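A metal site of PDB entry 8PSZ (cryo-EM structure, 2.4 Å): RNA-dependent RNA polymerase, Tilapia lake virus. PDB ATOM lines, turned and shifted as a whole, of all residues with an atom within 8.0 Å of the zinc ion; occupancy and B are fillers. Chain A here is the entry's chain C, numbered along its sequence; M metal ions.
The zinc ion is bound by NE2 of His 191 (2.0 Å), ND1 of His 184 (2.1 Å), SG of Cys 235 (2.3 Å) and SG of Cys 233 (2.3 Å).
N of His 184 lies within hydrogen-bond range of O of Ile 177, at 2.9 Å.
Within 4 Å of the zinc ion: His 184, His 191, Cys 233 and Cys 235. The nearest printed residue that does not touch the zinc ion is Pro 234 (4.7 Å).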
ATOM      1  N   PHE A 175     -17.236  -2.237  12.932  1.00  0.00           N
ATOM      2  CA  PHE A 175     -16.234  -1.484  12.193  1.00  0.00           C
ATOM      3  C   PHE A 175     -16.585  -0.008  12.167  1.00  0.00           C
ATOM      4  O   PHE A 175     -17.763   0.376  12.241  1.00  0.00           O
ATOM      5  CB  PHE A 175     -16.050  -2.019  10.773  1.00  0.00           C
ATOM      6  CG  PHE A 175     -17.241  -1.824   9.868  1.00  0.00           C
ATOM      7  CD1 PHE A 175     -17.500  -0.586   9.298  1.00  0.00           C
ATOM      8  CD2 PHE A 175     -18.085  -2.880   9.572  1.00  0.00           C
ATOM      9  CE1 PHE A 175     -18.596  -0.409   8.468  1.00  0.00           C
ATOM     10  CE2 PHE A 175     -19.171  -2.711   8.743  1.00  0.00           C
ATOM     11  CZ  PHE A 175     -19.427  -1.470   8.186  1.00  0.00           C
ATOM     12  N   ILE A 177     -15.605   3.259   9.625  1.00  0.00           N
ATOM     13  CA  ILE A 177     -15.033   3.607   8.331  1.00  0.00           C
ATOM     14  C   ILE A 177     -15.384   5.048   8.039  1.00  0.00           C
ATOM     15  O   ILE A 177     -16.270   5.636   8.653  1.00  0.00           O
ATOM     16  CB  ILE A 177     -15.534   2.660   7.215  1.00  0.00           C
ATOM     17  CG1 ILE A 177     -14.923   3.035   5.862  1.00  0.00           C
ATOM     18  CG2 ILE A 177     -17.058   2.655   7.157  1.00  0.00           C
ATOM     19  CD1 ILE A 177     -14.955   1.909   4.850  1.00  0.00           C
ATOM     20  N   ILE A 179     -16.578   7.599   5.056  1.00  0.00           N
ATOM     21  CA  ILE A 179     -17.148   7.787   3.728  1.00  0.00           C
ATOM     22  C   ILE A 179     -17.375   9.285   3.526  1.00  0.00           C
ATOM     23  O   ILE A 179     -18.034   9.935   4.350  1.00  0.00           O
ATOM     24  CB  ILE A 179     -18.466   7.010   3.550  1.00  0.00           C
ATOM     25  CG1 ILE A 179     -18.215   5.507   3.682  1.00  0.00           C
ATOM     26  CG2 ILE A 179     -19.086   7.307   2.198  1.00  0.00           C
ATOM     27  CD1 ILE A 179     -18.381   4.979   5.085  1.00  0.00           C
ATOM     28  N   PHE A 182     -17.924  11.819   6.548  1.00  0.00           N
ATOM     29  CA  PHE A 182     -18.592  11.279   7.729  1.00  0.00           C
ATOM     30  C   PHE A 182     -17.932   9.971   8.132  1.00  0.00           C
ATOM     31  O   PHE A 182     -17.282   9.298   7.337  1.00  0.00           O
ATOM     32  CB  PHE A 182     -20.089  11.043   7.463  1.00  0.00           C
ATOM     33  CG  PHE A 182     -20.860  12.311   7.216  1.00  0.00           C
ATOM     34  CD1 PHE A 182     -20.851  12.914   5.971  1.00  0.00           C
ATOM     35  CD2 PHE A 182     -21.602  12.900   8.231  1.00  0.00           C
ATOM     36  CE1 PHE A 182     -21.562  14.075   5.738  1.00  0.00           C
ATOM     37  CE2 PHE A 182     -22.306  14.059   8.005  1.00  0.00           C
ATOM     38  CZ  PHE A 182     -22.291  14.645   6.764  1.00  0.00           C
ATOM     39  N   TRP A 183     -18.107   9.628   9.412  1.00  0.00           N
ATOM     40  CA  TRP A 183     -17.592   8.386   9.973  1.00  0.00           C
ATOM     41  C   TRP A 183     -18.778   7.478  10.273  1.00  0.00           C
ATOM     42  O   TRP A 183     -19.583   7.777  11.162  1.00  0.00           O
ATOM     43  CB  TRP A 183     -16.771   8.649  11.228  1.00  0.00           C
ATOM     44  CG  TRP A 183     -15.460   9.304  10.965  1.00  0.00           C
ATOM     45  CD1 TRP A 183     -15.194  10.641  10.924  1.00  0.00           C
ATOM     46  CD2 TRP A 183     -14.214   8.649  10.699  1.00  0.00           C
ATOM     47  NE1 TRP A 183     -13.871  10.860  10.651  1.00  0.00           N
ATOM     48  CE2 TRP A 183     -13.239   9.655  10.503  1.00  0.00           C
ATOM     49  CE3 TRP A 183     -13.823   7.317  10.595  1.00  0.00           C
ATOM     50  CZ2 TRP A 183     -11.915   9.367  10.217  1.00  0.00           C
ATOM     51  CZ3 TRP A 183     -12.505   7.022  10.312  1.00  0.00           C
ATOM     52  CH2 TRP A 183     -11.563   8.044  10.126  1.00  0.00           C
ATOM     53  N   HIS A 184     -18.882   6.373   9.550  1.00  0.00           N
ATOM     54  CA  HIS A 184     -19.938   5.401   9.738  1.00  0.00           C
ATOM     55  C   HIS A 184     -19.449   4.288  10.657  1.00  0.00           C
ATOM     56  O   HIS A 184     -18.403   3.688  10.408  1.00  0.00           O
ATOM     57  CB  HIS A 184     -20.383   4.815   8.401  1.00  0.00           C
ATOM     58  CG  HIS A 184     -20.966   5.819   7.459  1.00  0.00           C
ATOM     59  ND1 HIS A 184     -22.141   5.596   6.768  1.00  0.00           N
ATOM     60  CD2 HIS A 184     -20.556   7.055   7.098  1.00  0.00           C
ATOM     61  CE1 HIS A 184     -22.407   6.650   6.014  1.00  0.00           C
ATOM     62  NE2 HIS A 184     -21.462   7.548   6.203  1.00  0.00           N
ATOM     63  N   MET A 185     -20.220   4.018  11.712  1.00  0.00           N
ATOM     64  CA  MET A 185     -19.950   2.934  12.643  1.00  0.00           C
ATOM     65  C   MET A 185     -21.066   1.907  12.530  1.00  0.00           C
ATOM     66  O   MET A 185     -22.243   2.258  12.693  1.00  0.00           O
ATOM     67  CB  MET A 185     -19.846   3.448  14.074  1.00  0.00           C
ATOM     68  CG  MET A 185     -18.763   4.501  14.290  1.00  0.00           C
ATOM     69  SD  MET A 185     -19.345   5.884  15.288  1.00  0.00           S
ATOM     70  CE  MET A 185     -19.984   6.967  14.019  1.00  0.00           C
ATOM     71  N   TYR A 186     -20.703   0.655  12.265  1.00  0.00           N
ATOM     72  CA  TYR A 186     -21.685  -0.417  12.102  1.00  0.00           C
ATOM     73  C   TYR A 186     -21.295  -1.601  12.975  1.00  0.00           C
ATOM     74  O   TYR A 186     -20.159  -2.063  12.927  1.00  0.00           O
ATOM     75  CB  TYR A 186     -21.801  -0.855  10.640  1.00  0.00           C
ATOM     76  CG  TYR A 186     -22.979  -1.776  10.366  1.00  0.00           C
ATOM     77  CD1 TYR A 186     -24.164  -1.668  11.090  1.00  0.00           C
ATOM     78  CD2 TYR A 186     -22.896  -2.754   9.386  1.00  0.00           C
ATOM     79  CE1 TYR A 186     -25.233  -2.505  10.843  1.00  0.00           C
ATOM     80  CE2 TYR A 186     -23.966  -3.605   9.135  1.00  0.00           C
ATOM     81  CZ  TYR A 186     -25.131  -3.470   9.864  1.00  0.00           C
ATOM     82  OH  TYR A 186     -26.183  -4.309   9.614  1.00  0.00           O
ATOM     83  N   HIS A 191     -26.424   1.211  13.201  1.00  0.00           N
ATOM     84  CA  HIS A 191     -25.582   1.953  12.280  1.00  0.00           C
ATOM     85  C   HIS A 191     -25.684   3.438  12.611  1.00  0.00           C
ATOM     86  O   HIS A 191     -26.794   3.992  12.610  1.00  0.00           O
ATOM     87  CB  HIS A 191     -25.991   1.702  10.820  1.00  0.00           C
ATOM     88  CG  HIS A 191     -25.357   2.638   9.847  1.00  0.00           C
ATOM     89  ND1 HIS A 191     -25.866   3.888   9.563  1.00  0.00           N
ATOM     90  CD2 HIS A 191     -24.252   2.507   9.076  1.00  0.00           C
ATOM     91  CE1 HIS A 191     -25.107   4.477   8.664  1.00  0.00           C
ATOM     92  NE2 HIS A 191     -24.114   3.657   8.351  1.00  0.00           N
ATOM     93  N   PHE A 192     -24.553   4.067  12.889  1.00  0.00           N
ATOM     94  CA  PHE A 192     -24.516   5.467  13.281  1.00  0.00           C
ATOM     95  C   PHE A 192     -23.501   6.225  12.443  1.00  0.00           C
ATOM     96  O   PHE A 192     -22.618   5.634  11.815  1.00  0.00           O
ATOM     97  CB  PHE A 192     -24.183   5.619  14.779  1.00  0.00           C
ATOM     98  CG  PHE A 192     -25.309   5.238  15.689  1.00  0.00           C
ATOM     99  CD1 PHE A 192     -26.553   5.836  15.562  1.00  0.00           C
ATOM    100  CD2 PHE A 192     -25.127   4.282  16.672  1.00  0.00           C
ATOM    101  CE1 PHE A 192     -27.596   5.481  16.399  1.00  0.00           C
ATOM    102  CE2 PHE A 192     -26.167   3.931  17.522  1.00  0.00           C
ATOM    103  CZ  PHE A 192     -27.401   4.530  17.386  1.00  0.00           C
ATOM    104  N   VAL A 193     -23.646   7.552  12.443  1.00  0.00           N
ATOM    105  CA  VAL A 193     -22.771   8.440  11.695  1.00  0.00           C
ATOM    106  C   VAL A 193     -22.273   9.533  12.637  1.00  0.00           C
ATOM    107  O   VAL A 193     -23.020  10.023  13.485  1.00  0.00           O
ATOM    108  CB  VAL A 193     -23.484   9.057  10.477  1.00  0.00           C
ATOM    109  CG1 VAL A 193     -22.734  10.280   9.976  1.00  0.00           C
ATOM    110  CG2 VAL A 193     -23.607   8.020   9.372  1.00  0.00           C
ATOM    111  N   ALA A 230     -26.052  11.160   6.989  1.00  0.00           N
ATOM    112  CA  ALA A 230     -25.330  10.997   5.736  1.00  0.00           C
ATOM    113  C   ALA A 230     -26.289  10.624   4.606  1.00  0.00           C
ATOM    114  O   ALA A 230     -27.441  10.257   4.838  1.00  0.00           O
ATOM    115  CB  ALA A 230     -24.237   9.925   5.870  1.00  0.00           C
ATOM    116  N   GLU A 232     -25.204   8.656   1.314  1.00  0.00           N
ATOM    117  CA  GLU A 232     -24.928   7.327   0.810  1.00  0.00           C
ATOM    118  C   GLU A 232     -24.156   6.532   1.853  1.00  0.00           C
ATOM    119  O   GLU A 232     -23.304   7.066   2.566  1.00  0.00           O
ATOM    120  CB  GLU A 232     -24.137   7.380  -0.500  1.00  0.00           C
ATOM    121  CG  GLU A 232     -24.980   7.758  -1.711  1.00  0.00           C
ATOM    122  CD  GLU A 232     -25.985   6.691  -2.086  1.00  0.00           C
ATOM    123  OE1 GLU A 232     -25.635   5.781  -2.865  1.00  0.00           O
ATOM    124  OE2 GLU A 232     -27.122   6.746  -1.579  1.00  0.00           O
ATOM    125  N   CYS A 233     -24.455   5.233   1.928  1.00  0.00           N
ATOM    126  CA  CYS A 233     -23.936   4.401   3.018  1.00  0.00           C
ATOM    127  C   CYS A 233     -23.878   2.939   2.623  1.00  0.00           C
ATOM    128  O   CYS A 233     -24.907   2.245   2.630  1.00  0.00           O
ATOM    129  CB  CYS A 233     -24.811   4.574   4.268  1.00  0.00           C
ATOM    130  SG  CYS A 233     -24.669   3.243   5.465  1.00  0.00           S
ATOM    131  N   PRO A 234     -22.676   2.401   2.300  1.00  0.00           N
ATOM    132  CA  PRO A 234     -22.554   1.023   1.874  1.00  0.00           C
ATOM    133  C   PRO A 234     -22.266   0.123   3.082  1.00  0.00           C
ATOM    134  O   PRO A 234     -21.802  -0.929   2.854  1.00  0.00           O
ATOM    135  CB  PRO A 234     -21.363   1.142   0.925  1.00  0.00           C
ATOM    136  CG  PRO A 234     -20.435   2.086   1.653  1.00  0.00           C
ATOM    137  CD  PRO A 234     -21.374   3.079   2.321  1.00  0.00           C
ATOM    138  N   CYS A 235     -22.577   0.552   4.307  1.00  0.00           N
ATOM    139  CA  CYS A 235     -22.237  -0.223   5.499  1.00  0.00           C
ATOM    140  C   CYS A 235     -22.752  -1.651   5.415  1.00  0.00           C
ATOM    141  O   CYS A 235     -22.068  -2.594   5.822  1.00  0.00           O
ATOM    142  CB  CYS A 235     -22.768   0.476   6.745  1.00  0.00           C
ATOM    143  SG  CYS A 235     -21.686   1.758   7.394  1.00  0.00           S
ATOM    144  N   LYS A 236     -23.970  -1.827   4.906  1.00  0.00           N
ATOM    145  CA  LYS A 236     -24.527  -3.182   4.790  1.00  0.00           C
ATOM    146  C   LYS A 236     -23.697  -4.038   3.843  1.00  0.00           C
ATOM    147  O   LYS A 236     -23.338  -5.180   4.173  1.00  0.00           O
ATOM    148  CB  LYS A 236     -25.976  -3.102   4.307  1.00  0.00           C
ATOM    149  CG  LYS A 236     -26.922  -2.395   5.251  1.00  0.00           C
ATOM    150  CD  LYS A 236     -28.304  -2.251   4.622  1.00  0.00           C
ATOM    151  CE  LYS A 236     -29.316  -1.699   5.615  1.00  0.00           C
ATOM    152  NZ  LYS A 236     -30.616  -1.368   4.949  1.00  0.00           N
ATOM    153  N   VAL A 238     -20.505  -3.655   2.767  1.00  0.00           N
ATOM    154  CA  VAL A 238     -19.174  -3.947   3.285  1.00  0.00           C
ATOM    155  C   VAL A 238     -19.258  -4.900   4.464  1.00  0.00           C
ATOM    156  O   VAL A 238     -18.370  -5.751   4.657  1.00  0.00           O
ATOM    157  CB  VAL A 238     -18.441  -2.642   3.661  1.00  0.00           C
ATOM    158  CG1 VAL A 238     -18.437  -1.676   2.493  1.00  0.00           C
ATOM    159  CG2 VAL A 238     -19.086  -1.997   4.881  1.00  0.00           C
HETATM  160 ZN    ZN M   1     -22.824   3.662   6.783  1.00  0.00          ZN
